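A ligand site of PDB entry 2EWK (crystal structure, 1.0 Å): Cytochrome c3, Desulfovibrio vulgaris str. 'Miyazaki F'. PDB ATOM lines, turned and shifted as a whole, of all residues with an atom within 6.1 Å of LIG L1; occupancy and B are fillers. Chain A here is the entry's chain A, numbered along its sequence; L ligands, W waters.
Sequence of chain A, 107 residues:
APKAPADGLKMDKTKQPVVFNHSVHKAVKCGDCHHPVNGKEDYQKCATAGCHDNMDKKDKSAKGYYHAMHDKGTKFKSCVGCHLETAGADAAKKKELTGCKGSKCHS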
ATOM      1  N   MET A  11       9.962   6.741 -14.030  1.00  0.00           N
ATOM      2  CA  MET A  11      11.007   6.672 -12.997  1.00  0.00           C
ATOM      3  C   MET A  11      12.302   6.721 -13.790  1.00  0.00           C
ATOM      4  O   MET A  11      12.593   5.838 -14.570  1.00  0.00           O
ATOM      5  CB  MET A  11      10.839   5.385 -12.232  1.00  0.00           C
ATOM      6  CG  MET A  11       9.495   5.280 -11.526  1.00  0.00           C
ATOM      7  SD  MET A  11       9.253   3.698 -10.671  1.00  0.00           S
ATOM      8  CE  MET A  11      10.334   3.944  -9.258  1.00  0.00           C
ATOM      9  N   ASP A  12      13.057   7.845 -13.600  1.00  0.00           N
ATOM     10  CA  ASP A  12      14.200   8.083 -14.497  1.00  0.00           C
ATOM     11  C   ASP A  12      15.402   8.603 -13.759  1.00  0.00           C
ATOM     12  O   ASP A  12      16.141   9.464 -14.247  1.00  0.00           O
ATOM     13  CB  ASP A  12      13.768   9.044 -15.603  1.00  0.00           C
ATOM     14  CG  ASP A  12      13.247  10.370 -15.068  1.00  0.00           C
ATOM     15  OD1 ASP A  12      13.404  10.708 -13.861  1.00  0.00           O
ATOM     16  OD2 ASP A  12      12.700  11.170 -15.880  1.00  0.00           O
ATOM     17  N   LYS A  13      15.669   8.008 -12.595  1.00  0.00           N
ATOM     18  CA  LYS A  13      16.902   8.287 -11.898  1.00  0.00           C
ATOM     19  C   LYS A  13      18.130   7.656 -12.501  1.00  0.00           C
ATOM     20  O   LYS A  13      19.266   8.012 -12.184  1.00  0.00           O
ATOM     21  CB  LYS A  13      16.822   7.764 -10.456  1.00  0.00           C
ATOM     22  CG  LYS A  13      15.635   8.302  -9.666  1.00  0.00           C
ATOM     23  CD  LYS A  13      15.461   9.754  -9.612  1.00  0.00           C
ATOM     24  CE  LYS A  13      16.584  10.466  -8.880  1.00  0.00           C
ATOM     25  NZ  LYS A  13      16.214  11.892  -8.599  1.00  0.00           N
ATOM     26  N   THR A  14      17.926   6.672 -13.396  1.00  0.00           N
ATOM     27  CA  THR A  14      18.973   5.849 -13.959  1.00  0.00           C
ATOM     28  C   THR A  14      18.909   5.854 -15.488  1.00  0.00           C
ATOM     29  O   THR A  14      17.973   6.445 -16.061  1.00  0.00           O
ATOM     30  CB  THR A  14      18.876   4.386 -13.496  1.00  0.00           C
ATOM     31  OG1 THR A  14      17.874   3.674 -14.265  1.00  0.00           O
ATOM     32  CG2 THR A  14      18.559   4.265 -11.996  1.00  0.00           C
ATOM     33  N   LYS A  15      19.876   5.198 -16.112  1.00  0.00           N
ATOM     34  CA  LYS A  15      19.910   5.046 -17.567  1.00  0.00           C
ATOM     35  C   LYS A  15      18.993   3.894 -18.047  1.00  0.00           C
ATOM     36  O   LYS A  15      18.917   3.651 -19.278  1.00  0.00           O
ATOM     37  CB  LYS A  15      21.302   4.799 -18.096  1.00  0.00           C
ATOM     38  CG  LYS A  15      22.114   6.103 -17.937  1.00  0.00           C
ATOM     39  CD  LYS A  15      23.467   5.954 -18.576  1.00  0.00           C
ATOM     40  CE  LYS A  15      24.442   7.068 -18.191  1.00  0.00           C
ATOM     41  NZ  LYS A  15      25.759   6.848 -18.838  1.00  0.00           N
ATOM     42  N   GLN A  16      18.243   3.303 -17.094  1.00  0.00           N
ATOM     43  CA  GLN A  16      17.259   2.256 -17.461  1.00  0.00           C
ATOM     44  C   GLN A  16      15.874   2.700 -16.928  1.00  0.00           C
ATOM     45  O   GLN A  16      15.315   2.045 -16.055  1.00  0.00           O
ATOM     46  CB  GLN A  16      17.658   0.899 -16.896  1.00  0.00           C
ATOM     47  CG  GLN A  16      19.126   0.503 -17.213  1.00  0.00           C
ATOM     48  CD  GLN A  16      19.477   0.430 -18.642  1.00  0.00           C
ATOM     49  OE1 GLN A  16      18.583   0.150 -19.468  1.00  0.00           O
ATOM     50  NE2 GLN A  16      20.743   0.622 -18.992  1.00  0.00           N
ATOM     51  N   PRO A  17      15.324   3.785 -17.452  1.00  0.00           N
ATOM     52  CA  PRO A  17      14.078   4.349 -16.884  1.00  0.00           C
ATOM     53  C   PRO A  17      12.894   3.360 -17.098  1.00  0.00           C
ATOM     54  O   PRO A  17      12.835   2.597 -18.077  1.00  0.00           O
ATOM     55  CB  PRO A  17      13.887   5.615 -17.653  1.00  0.00           C
ATOM     56  CG  PRO A  17      14.672   5.421 -18.916  1.00  0.00           C
ATOM     57  CD  PRO A  17      15.853   4.610 -18.587  1.00  0.00           C
ATOM     58  N   VAL A  18      11.941   3.474 -16.169  1.00  0.00           N
ATOM     59  CA  VAL A  18      10.772   2.563 -16.145  1.00  0.00           C
ATOM     60  C   VAL A  18       9.492   3.346 -15.973  1.00  0.00           C
ATOM     61  O   VAL A  18       9.454   4.270 -15.135  1.00  0.00           O
ATOM     62  CB  VAL A  18      10.972   1.529 -15.001  1.00  0.00           C
ATOM     63  CG1 VAL A  18       9.733   0.650 -14.847  1.00  0.00           C
ATOM     64  CG2 VAL A  18      12.218   0.684 -15.261  1.00  0.00           C
ATOM     65  N   MET A  55      22.642   5.694  -5.337  1.00  0.00           N
ATOM     66  CA  MET A  55      22.536   5.244  -6.737  1.00  0.00           C
ATOM     67  C   MET A  55      23.602   4.207  -7.102  1.00  0.00           C
ATOM     68  O   MET A  55      23.806   3.908  -8.289  1.00  0.00           O
ATOM     69  CB  MET A  55      22.571   6.467  -7.651  1.00  0.00           C
ATOM     70  CG  MET A  55      21.310   7.299  -7.566  1.00  0.00           C
ATOM     71  SD  MET A  55      19.830   6.441  -8.115  1.00  0.00           S
ATOM     72  CE  MET A  55      18.593   7.193  -7.113  1.00  0.00           C
ATOM     73  N   ASP A  56      24.257   3.629  -6.079  1.00  0.00           N
ATOM     74  CA  ASP A  56      25.099   2.446  -6.320  1.00  0.00           C
ATOM     75  C   ASP A  56      24.194   1.203  -6.324  1.00  0.00           C
ATOM     76  O   ASP A  56      23.648   0.852  -5.291  1.00  0.00           O
ATOM     77  CB  ASP A  56      26.174   2.296  -5.286  1.00  0.00           C
ATOM     78  CG  ASP A  56      27.081   1.117  -5.727  1.00  0.00           C
ATOM     79  OD1 ASP A  56      26.736   0.005  -5.653  1.00  0.00           O
ATOM     80  OD2 ASP A  56      28.217   1.275  -6.274  1.00  0.00           O
ATOM     81  N   LYS A  57      24.101   0.585  -7.500  1.00  0.00           N
ATOM     82  CA  LYS A  57      23.156  -0.547  -7.677  1.00  0.00           C
ATOM     83  C   LYS A  57      23.525  -1.791  -6.909  1.00  0.00           C
ATOM     84  O   LYS A  57      22.692  -2.705  -6.892  1.00  0.00           O
ATOM     85  CB  LYS A  57      22.885  -0.830  -9.159  1.00  0.00           C
ATOM     86  CG  LYS A  57      24.019  -1.482  -9.885  1.00  0.00           C
ATOM     87  CD  LYS A  57      23.656  -1.744 -11.366  1.00  0.00           C
ATOM     88  CE  LYS A  57      24.922  -2.101 -12.178  1.00  0.00           C
ATOM     89  NZ  LYS A  57      24.494  -2.336 -13.600  1.00  0.00           N
ATOM     90  N   TYR A  65      18.688   2.559  -3.954  1.00  0.00           N
ATOM     91  CA  TYR A  65      17.556   2.696  -4.875  1.00  0.00           C
ATOM     92  C   TYR A  65      17.311   1.417  -5.654  1.00  0.00           C
ATOM     93  O   TYR A  65      16.145   0.923  -5.746  1.00  0.00           O
ATOM     94  CB  TYR A  65      17.823   3.901  -5.764  1.00  0.00           C
ATOM     95  CG  TYR A  65      16.741   4.233  -6.734  1.00  0.00           C
ATOM     96  CD1 TYR A  65      16.884   3.975  -8.100  1.00  0.00           C
ATOM     97  CD2 TYR A  65      15.553   4.855  -6.337  1.00  0.00           C
ATOM     98  CE1 TYR A  65      15.886   4.315  -9.007  1.00  0.00           C
ATOM     99  CE2 TYR A  65      14.575   5.201  -7.248  1.00  0.00           C
ATOM    100  CZ  TYR A  65      14.732   4.921  -8.576  1.00  0.00           C
ATOM    101  OH  TYR A  65      13.732   5.256  -9.470  1.00  0.00           O
ATOM    102  N   TYR A  66      18.331   0.863  -6.280  1.00  0.00           N
ATOM    103  CA  TYR A  66      18.161  -0.379  -7.023  1.00  0.00           C
ATOM    104  C   TYR A  66      17.583  -1.459  -6.115  1.00  0.00           C
ATOM    105  O   TYR A  66      16.671  -2.215  -6.506  1.00  0.00           O
ATOM    106  CB  TYR A  66      19.529  -0.809  -7.605  1.00  0.00           C
ATOM    107  CG  TYR A  66      19.452  -2.118  -8.399  1.00  0.00           C
ATOM    108  CD1 TYR A  66      19.488  -3.351  -7.758  1.00  0.00           C
ATOM    109  CD2 TYR A  66      19.331  -2.114  -9.787  1.00  0.00           C
ATOM    110  CE1 TYR A  66      19.412  -4.539  -8.465  1.00  0.00           C
ATOM    111  CE2 TYR A  66      19.255  -3.317 -10.485  1.00  0.00           C
ATOM    112  CZ  TYR A  66      19.288  -4.501  -9.832  1.00  0.00           C
ATOM    113  OH  TYR A  66      19.210  -5.681 -10.590  1.00  0.00           O
ATOM    114  N   MET A  69      13.859  -1.507  -5.569  1.00  0.00           N
ATOM    115  CA  MET A  69      13.011  -1.854  -6.708  1.00  0.00           C
ATOM    116  C   MET A  69      13.144  -3.315  -7.112  1.00  0.00           C
ATOM    117  O   MET A  69      12.237  -3.833  -7.781  1.00  0.00           O
ATOM    118  CB  MET A  69      13.341  -0.975  -7.943  1.00  0.00           C
ATOM    119  CG  MET A  69      13.305   0.521  -7.655  1.00  0.00           C
ATOM    120  SD  MET A  69      11.747   1.065  -6.920  1.00  0.00           S
ATOM    121  CE  MET A  69      12.260   2.673  -6.311  1.00  0.00           C
ATOM    122  N   HIS A  70      14.241  -3.992  -6.728  1.00  0.00           N
ATOM    123  CA  HIS A  70      14.553  -5.297  -7.309  1.00  0.00           C
ATOM    124  C   HIS A  70      14.620  -6.451  -6.337  1.00  0.00           C
ATOM    125  O   HIS A  70      14.507  -7.626  -6.813  1.00  0.00           O
ATOM    126  CB  HIS A  70      15.894  -5.278  -8.080  1.00  0.00           C
ATOM    127  CG  HIS A  70      15.877  -4.345  -9.304  1.00  0.00           C
ATOM    128  ND1 HIS A  70      16.140  -3.010  -9.150  1.00  0.00           N
ATOM    129  CD2 HIS A  70      15.623  -4.551 -10.602  1.00  0.00           C
ATOM    130  CE1 HIS A  70      16.043  -2.434 -10.354  1.00  0.00           C
ATOM    131  NE2 HIS A  70      15.714  -3.350 -11.277  1.00  0.00           N
ATOM    132  N   CYS A  79       9.247  -3.870  -6.414  1.00  0.00           N
ATOM    133  CA  CYS A  79       8.619  -4.119  -7.696  1.00  0.00           C
ATOM    134  C   CYS A  79       8.831  -5.603  -8.103  1.00  0.00           C
ATOM    135  O   CYS A  79       7.863  -6.317  -8.412  1.00  0.00           O
ATOM    136  CB  CYS A  79       9.244  -3.281  -8.804  1.00  0.00           C
ATOM    137  SG  CYS A  79       9.539  -1.507  -8.457  1.00  0.00           S
ATOM    138  N   VAL A  80      10.072  -6.014  -8.152  1.00  0.00           N
ATOM    139  CA  VAL A  80      10.383  -7.369  -8.661  1.00  0.00           C
ATOM    140  C   VAL A  80       9.877  -8.401  -7.660  1.00  0.00           C
ATOM    141  O   VAL A  80       9.345  -9.449  -8.078  1.00  0.00           O
ATOM    142  CB  VAL A  80      11.863  -7.549  -8.990  1.00  0.00           C
ATOM    143  CG1 VAL A  80      12.218  -8.988  -9.392  1.00  0.00           C
ATOM    144  CG2 VAL A  80      12.320  -6.604 -10.083  1.00  0.00           C
ATOM    145  N   HIS A  83       6.184  -8.788  -8.108  1.00  0.00           N
ATOM    146  CA  HIS A  83       5.915  -9.386  -9.396  1.00  0.00           C
ATOM    147  C   HIS A  83       6.282 -10.873  -9.434  1.00  0.00           C
ATOM    148  O   HIS A  83       5.562 -11.630 -10.132  1.00  0.00           O
ATOM    149  CB  HIS A  83       6.680  -8.622 -10.477  1.00  0.00           C
ATOM    150  CG  HIS A  83       6.036  -7.302 -10.815  1.00  0.00           C
ATOM    151  ND1 HIS A  83       6.385  -6.682 -11.992  1.00  0.00           N
ATOM    152  CD2 HIS A  83       5.140  -6.501 -10.212  1.00  0.00           C
ATOM    153  CE1 HIS A  83       5.720  -5.527 -12.024  1.00  0.00           C
ATOM    154  NE2 HIS A  83       4.934  -5.351 -10.974  1.00  0.00           N
ATOM    155  N   GLU A  96       7.368 -11.338 -18.572  1.00  0.00           N
ATOM    156  CA  GLU A  96       6.715 -10.057 -18.697  1.00  0.00           C
ATOM    157  C   GLU A  96       6.930  -9.164 -17.471  1.00  0.00           C
ATOM    158  O   GLU A  96       7.097  -7.952 -17.549  1.00  0.00           O
ATOM    159  CB  GLU A  96       5.206 -10.278 -18.835  1.00  0.00           C
ATOM    160  CG  GLU A  96       4.730 -10.761 -20.153  1.00  0.00           C
ATOM    161  CD  GLU A  96       3.203 -10.985 -20.064  1.00  0.00           C
ATOM    162  OE1 GLU A  96       2.521 -10.307 -19.227  1.00  0.00           O
ATOM    163  OE2 GLU A  96       2.713 -11.866 -20.779  1.00  0.00           O
ATOM    164  N   LEU A  97       6.799  -9.765 -16.263  1.00  0.00           N
ATOM    165  CA  LEU A  97       6.739  -8.994 -15.038  1.00  0.00           C
ATOM    166  C   LEU A  97       8.055  -8.963 -14.295  1.00  0.00           C
ATOM    167  O   LEU A  97       8.243  -8.056 -13.440  1.00  0.00           O
ATOM    168  CB  LEU A  97       5.643  -9.615 -14.114  1.00  0.00           C
ATOM    169  CG  LEU A  97       4.248  -9.544 -14.654  1.00  0.00           C
ATOM    170  CD1 LEU A  97       3.281 -10.181 -13.606  1.00  0.00           C
ATOM    171  CD2 LEU A  97       3.779  -8.147 -14.995  1.00  0.00           C
ATOM    172  N   THR A  98       8.980  -9.906 -14.565  1.00  0.00           N
ATOM    173  CA  THR A  98      10.247  -9.969 -13.810  1.00  0.00           C
ATOM    174  C   THR A  98      11.473 -10.022 -14.695  1.00  0.00           C
ATOM    175  O   THR A  98      12.584  -9.948 -14.141  1.00  0.00           O
ATOM    176  CB  THR A  98      10.296 -11.120 -12.770  1.00  0.00           C
ATOM    177  OG1 THR A  98      10.472 -12.396 -13.402  1.00  0.00           O
ATOM    178  CG2 THR A  98       9.022 -11.111 -11.944  1.00  0.00           C
ATOM    179  N   GLY A  99      11.346 -10.095 -16.000  1.00  0.00           N
ATOM    180  CA  GLY A  99      12.527 -10.235 -16.861  1.00  0.00           C
ATOM    181  C   GLY A  99      13.387  -8.969 -16.774  1.00  0.00           C
ATOM    182  O   GLY A  99      12.925  -7.842 -16.718  1.00  0.00           O
ATOM    183  N   CYS A 100      14.707  -9.225 -16.863  1.00  0.00           N
ATOM    184  CA  CYS A 100      15.636  -8.075 -16.802  1.00  0.00           C
ATOM    185  C   CYS A 100      15.700  -7.315 -18.097  1.00  0.00           C
ATOM    186  O   CYS A 100      16.127  -6.167 -18.127  1.00  0.00           O
ATOM    187  CB  CYS A 100      17.066  -8.553 -16.468  1.00  0.00           C
ATOM    188  SG  CYS A 100      17.089  -9.570 -14.933  1.00  0.00           S
ATOM    189  N   LYS A 101      15.322  -7.942 -19.206  1.00  0.00           N
ATOM    190  CA  LYS A 101      15.244  -7.262 -20.528  1.00  0.00           C
ATOM    191  C   LYS A 101      14.027  -7.880 -21.191  1.00  0.00           C
ATOM    192  O   LYS A 101      13.590  -8.957 -20.836  1.00  0.00           O
ATOM    193  CB  LYS A 101      16.494  -7.357 -21.374  1.00  0.00           C
ATOM    194  CG  LYS A 101      16.722  -8.752 -21.859  1.00  0.00           C
ATOM    195  CD  LYS A 101      18.061  -8.815 -22.617  1.00  0.00           C
ATOM    196  CE  LYS A 101      18.261 -10.189 -23.233  1.00  0.00           C
ATOM    197  NZ  LYS A 101      17.400 -10.259 -24.445  1.00  0.00           N
ATOM    198  N   SER A 103      10.994  -7.086 -20.884  1.00  0.00           N
ATOM    199  CA  SER A 103       9.888  -7.189 -19.916  1.00  0.00           C
ATOM    200  C   SER A 103       9.076  -5.927 -19.977  1.00  0.00           C
ATOM    201  O   SER A 103       9.413  -4.985 -20.706  1.00  0.00           O
ATOM    202  CB  SER A 103      10.398  -7.451 -18.518  1.00  0.00           C
ATOM    203  OG  SER A 103      11.074  -6.269 -18.013  1.00  0.00           O
ATOM    204  N   LYS A 104       8.003  -5.874 -19.195  1.00  0.00           N
ATOM    205  CA  LYS A 104       7.196  -4.637 -19.159  1.00  0.00           C
ATOM    206  C   LYS A 104       7.906  -3.541 -18.434  1.00  0.00           C
ATOM    207  O   LYS A 104       7.507  -2.370 -18.569  1.00  0.00           O
ATOM    208  CB  LYS A 104       5.795  -4.891 -18.562  1.00  0.00           C
ATOM    209  CG  LYS A 104       5.007  -5.930 -19.369  1.00  0.00           C
ATOM    210  CD  LYS A 104       3.515  -5.717 -19.394  1.00  0.00           C
ATOM    211  CE  LYS A 104       3.007  -6.437 -20.633  1.00  0.00           C
ATOM    212  NZ  LYS A 104       2.350  -5.498 -21.567  1.00  0.00           N
ATOM    213  N   CYS A 105       8.920  -3.836 -17.638  1.00  0.00           N
ATOM    214  CA  CYS A 105       9.740  -2.784 -17.014  1.00  0.00           C
ATOM    215  C   CYS A 105      10.874  -2.310 -17.902  1.00  0.00           C
ATOM    216  O   CYS A 105      11.047  -1.093 -18.076  1.00  0.00           O
ATOM    217  CB  CYS A 105      10.320  -3.246 -15.683  1.00  0.00           C
ATOM    218  SG  CYS A 105       8.983  -3.665 -14.521  1.00  0.00           S
ATOM    219  N   HIS A 106      11.645  -3.261 -18.452  1.00  0.00           N
ATOM    220  CA  HIS A 106      12.804  -2.914 -19.251  1.00  0.00           C
ATOM    221  C   HIS A 106      12.681  -3.516 -20.636  1.00  0.00           C
ATOM    222  O   HIS A 106      12.659  -4.732 -20.801  1.00  0.00           O
ATOM    223  CB  HIS A 106      14.084  -3.485 -18.622  1.00  0.00           C
ATOM    224  CG  HIS A 106      14.427  -2.925 -17.244  1.00  0.00           C
ATOM    225  ND1 HIS A 106      14.638  -1.612 -17.011  1.00  0.00           N
ATOM    226  CD2 HIS A 106      14.620  -3.541 -16.049  1.00  0.00           C
ATOM    227  CE1 HIS A 106      14.952  -1.464 -15.694  1.00  0.00           C
ATOM    228  NE2 HIS A 106      14.973  -2.621 -15.092  1.00  0.00           N
HETATM  229  C1  LIG L   1      16.597   0.202 -12.888  1.00  0.00           C
HETATM  230  C2  LIG L   1      18.521  -4.118 -13.909  1.00  0.00           C
HETATM  231  C3  LIG L   1      14.188  -6.150 -13.679  1.00  0.00           C
HETATM  232  C4  LIG L   1      12.303  -1.904 -12.295  1.00  0.00           C
HETATM  233  C5  LIG L   1      17.480  -0.795 -13.304  1.00  0.00           C
HETATM  234  C6  LIG L   1      18.852  -0.518 -13.634  1.00  0.00           C
HETATM  235  C7  LIG L   1      19.387  -1.797 -13.936  1.00  0.00           C
HETATM  236  C8  LIG L   1      18.337  -2.731 -13.805  1.00  0.00           C
HETATM  237  C9  LIG L   1      20.818  -2.149 -14.307  1.00  0.00           C
HETATM  238  C10 LIG L   1      19.609   0.731 -13.570  1.00  0.00           C
HETATM  239  C11 LIG L   1      20.406   0.820 -12.247  1.00  0.00           C
HETATM  240  C12 LIG L   1      21.415   2.002 -12.221  1.00  0.00           C
HETATM  241  O1  LIG L   1      22.154   2.145 -13.216  1.00  0.00           O
HETATM  242  O2  LIG L   1      21.424   2.767 -11.253  1.00  0.00           O
HETATM  243  C13 LIG L   1      17.530  -5.059 -13.777  1.00  0.00           C
HETATM  244  C14 LIG L   1      17.759  -6.455 -13.827  1.00  0.00           C
HETATM  245  C15 LIG L   1      16.533  -7.074 -13.744  1.00  0.00           C
HETATM  246  C16 LIG L   1      15.555  -6.003 -13.672  1.00  0.00           C
HETATM  247  C17 LIG L   1      19.167  -7.060 -13.865  1.00  0.00           C
HETATM  248  C18 LIG L   1      16.188  -8.494 -13.725  1.00  0.00           C
HETATM  249  C19 LIG L   1      16.418  -9.134 -12.353  1.00  0.00           C
HETATM  250  C20 LIG L   1      13.293  -5.140 -13.449  1.00  0.00           C
HETATM  251  C21 LIG L   1      11.880  -5.304 -13.473  1.00  0.00           C
HETATM  252  C22 LIG L   1      11.321  -4.110 -13.047  1.00  0.00           C
HETATM  253  C23 LIG L   1      12.422  -3.238 -12.809  1.00  0.00           C
HETATM  254  C24 LIG L   1      11.167  -6.587 -13.937  1.00  0.00           C
HETATM  255  C25 LIG L   1       9.875  -3.748 -12.887  1.00  0.00           C
HETATM  256  C26 LIG L   1       9.063  -4.724 -12.000  1.00  0.00           C
HETATM  257  C27 LIG L   1      13.331  -1.026 -12.206  1.00  0.00           C
HETATM  258  C28 LIG L   1      13.157   0.337 -11.745  1.00  0.00           C
HETATM  259  C29 LIG L   1      14.369   0.953 -11.975  1.00  0.00           C
HETATM  260  C30 LIG L   1      15.247  -0.037 -12.556  1.00  0.00           C
HETATM  261  C31 LIG L   1      11.917   0.924 -11.205  1.00  0.00           C
HETATM  262  C32 LIG L   1      14.702   2.432 -11.751  1.00  0.00           C
HETATM  263  C33 LIG L   1      14.295   3.306 -12.958  1.00  0.00           C
HETATM  264  C34 LIG L   1      14.864   4.692 -12.884  1.00  0.00           C
HETATM  265  O3  LIG L   1      14.557   5.429 -11.903  1.00  0.00           O
HETATM  266  O4  LIG L   1      15.663   5.039 -13.800  1.00  0.00           O
HETATM  267  N1  LIG L   1      17.145  -2.117 -13.420  1.00  0.00           N
HETATM  268  N2  LIG L   1      16.189  -4.777 -13.626  1.00  0.00           N
HETATM  269  N3  LIG L   1      13.632  -3.848 -13.078  1.00  0.00           N
HETATM  270  N4  LIG L   1      14.624  -1.237 -12.660  1.00  0.00           N
HETATM  271 FE1  LIG L   1      15.395  -2.993 -13.203  1.00  0.00          FE
HETATM  272  C1  LG2 L   2       1.928  -4.932 -13.302  1.00  0.00           C
HETATM  273  C2  LG2 L   2       5.726  -2.010 -12.782  1.00  0.00           C
HETATM  274  C3  LG2 L   2       5.516  -2.627  -8.001  1.00  0.00           C
HETATM  275  C4  LG2 L   2       1.886  -5.752  -8.513  1.00  0.00           C
HETATM  276  C5  LG2 L   2       2.962  -4.088 -13.554  1.00  0.00           C
HETATM  277  C6  LG2 L   2       3.419  -3.746 -14.909  1.00  0.00           C
HETATM  278  C7  LG2 L   2       4.469  -2.889 -14.750  1.00  0.00           C
HETATM  279  C8  LG2 L   2       4.669  -2.751 -13.338  1.00  0.00           C
HETATM  280  C9  LG2 L   2       5.324  -2.233 -15.807  1.00  0.00           C
HETATM  281  C10 LG2 L   2       2.706  -4.211 -16.169  1.00  0.00           C
HETATM  282  C11 LG2 L   2       1.521  -3.313 -16.585  1.00  0.00           C
HETATM  283  C12 LG2 L   2       1.930  -1.933 -16.891  1.00  0.00           C
HETATM  284  O1  LG2 L   2       2.536  -1.674 -18.017  1.00  0.00           O
HETATM  285  O2  LG2 L   2       1.747  -1.039 -16.068  1.00  0.00           O
HETATM  286  C13 LG2 L   2       5.971  -1.920 -11.417  1.00  0.00           C
HETATM  287  C14 LG2 L   2       7.073  -1.144 -10.866  1.00  0.00           C
HETATM  288  C15 LG2 L   2       6.992  -1.282  -9.516  1.00  0.00           C
HETATM  289  C16 LG2 L   2       5.855  -2.174  -9.291  1.00  0.00           C
HETATM  290  C17 LG2 L   2       8.085  -0.383 -11.694  1.00  0.00           C
HETATM  291  C18 LG2 L   2       7.858  -0.757  -8.427  1.00  0.00           C
HETATM  292  C19 LG2 L   2       8.022   0.785  -8.511  1.00  0.00           C
HETATM  293  C20 LG2 L   2       4.544  -3.584  -7.729  1.00  0.00           C
HETATM  294  C21 LG2 L   2       4.282  -4.117  -6.412  1.00  0.00           C
HETATM  295  C22 LG2 L   2       3.295  -5.019  -6.553  1.00  0.00           C
HETATM  296  C23 LG2 L   2       2.921  -5.030  -7.981  1.00  0.00           C
HETATM  297  C24 LG2 L   2       5.081  -3.665  -5.174  1.00  0.00           C
HETATM  298  C25 LG2 L   2       2.631  -5.925  -5.582  1.00  0.00           C
HETATM  299  C26 LG2 L   2       2.616  -5.443  -4.087  1.00  0.00           C
HETATM  300  C27 LG2 L   2       1.551  -5.759  -9.867  1.00  0.00           C
HETATM  301  C28 LG2 L   2       0.412  -6.439 -10.435  1.00  0.00           C
HETATM  302  C29 LG2 L   2       0.404  -6.201 -11.760  1.00  0.00           C
HETATM  303  C30 LG2 L   2       1.529  -5.351 -11.995  1.00  0.00           C
HETATM  304  C31 LG2 L   2      -0.531  -7.341  -9.597  1.00  0.00           C
HETATM  305  C32 LG2 L   2      -0.505  -6.782 -12.783  1.00  0.00           C
HETATM  306  C33 LG2 L   2       0.144  -8.116 -13.388  1.00  0.00           C
HETATM  307  C34 LG2 L   2      -0.362  -8.594 -14.653  1.00  0.00           C
HETATM  308  O3  LG2 L   2      -0.207  -9.703 -15.015  1.00  0.00           O
HETATM  309  O4  LG2 L   2      -1.116  -7.814 -15.374  1.00  0.00           O
HETATM  310  N1  LG2 L   2       3.747  -3.455 -12.603  1.00  0.00           N
HETATM  311  N2  LG2 L   2       5.273  -2.573 -10.439  1.00  0.00           N
HETATM  312  N3  LG2 L   2       3.728  -4.168  -8.685  1.00  0.00           N
HETATM  313  N4  LG2 L   2       2.188  -5.038 -10.861  1.00  0.00           N
HETATM  314 FE1  LG2 L   2       3.728  -3.819 -10.644  1.00  0.00          FE
HETATM  315  O   HOH W   1      22.976  -4.753 -13.567  1.00  0.00           O
HETATM  316  O   HOH W   2      22.829   4.885 -10.688  1.00  0.00           O
HETATM  317  O   HOH W   3      22.252   4.271 -14.819  1.00  0.00           O
HETATM  318  O   HOH W   4      20.214   3.092  -8.817  1.00  0.00           O
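The backbone carbonyl oxygen (O) of Met 11 sits close to an oxygen (O4) of LIG L1, at 3.3 Å. Residues that only touch LIG L1: Gln 16 (3.5 Å), Pro 17 (3.5 Å), Val 18 (3.7 Å), Met 55 (3.97 Å), Lys 57 (3.7 Å), Tyr 66 (3.5 Å), Met 69 (3.8 Å), Cys 79 (3.5 Å), Val 80 (3.7 Å), His 83 (3.3 Å), Leu 97 (3.3 Å), Thr 98 (3.5 Å) and Gly 99 (3.5 Å). The nearest printed residue that does not touch LIG L1 is Ser 103 (4.1 Å).
OG of Ser 103 sits close to N of Cys 105, 3.3 Å away. N of His 106 sits at hydrogen-bond distance from OG of Ser 103 (3.1 Å). ND1 of His 70 sits at hydrogen-bond distance from O of Tyr 66, 2.8 Å away. OG1 of Thr 14 sits at hydrogen-bond distance from N of Gln 16 (2.9 Å). O of Val 18 lies within hydrogen-bond range of N of Met 11, at 2.8 Å. A ring nitrogen (ND1) of His 83 sits at hydrogen-bond distance from the backbone carbonyl oxygen (O) of Leu 97 (2.7 Å). O of Gly 99 is in hydrogen-bond range of OG of Ser 103. N of Val 80 lies within hydrogen-bond range of O of Met 69 (3.1 Å).
Water W2 lies within hydrogen-bond range of O2 of LIG L1 (2.6 Å) and O of Met 55 (2.8 Å). Water W3 bridges an oxygen (O1) of LIG L1 (2.7 Å) and the backbone NH (N) of Lys 15 (2.9 Å). Water W4 bridges O2 of LIG L1 and SD of Met 55.
The side-chain sulfur (SG) of Cys 100 is covalently linked to a carbon (C18) of LIG L1, 1.9 Å away. C25 of LIG L1 is covalently linked to SG of Cys 105 (1.9 Å). A ring nitrogen (NE2) of His 106 binds an iron atom (FE1) of LIG L1, 2.0 Å away. An iron atom (FE1) of LIG L1 is bound by a ring nitrogen (NE2) of His 70, at 2.0 Å. O3 of LIG L1 lies within hydrogen-bond range of OH of Tyr 65 (2.6 Å). An oxygen (O4) of LIG L1 lies within hydrogen-bond range of the backbone NH (N) of Thr 14, 2.8 Å away. O4 of LIG L1 sits at hydrogen-bond distance from OG1 of Thr 14 (2.6 Å). An oxygen (O3) of LIG L1 is in hydrogen-bond range of the backbone NH (N) of Lys 13, 2.9 Å away. The backbone NH (N) of Asp 12 lies within hydrogen-bond range of an oxygen (O3) of LIG L1 (3.3 Å). NE2 of His 83 is bound to FE1 of LG2 L2, at 2.0 Å. The side-chain sulfur (SG) of Cys 79 is covalently linked to a carbon (C18) of LG2 L2 (1.8 Å).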
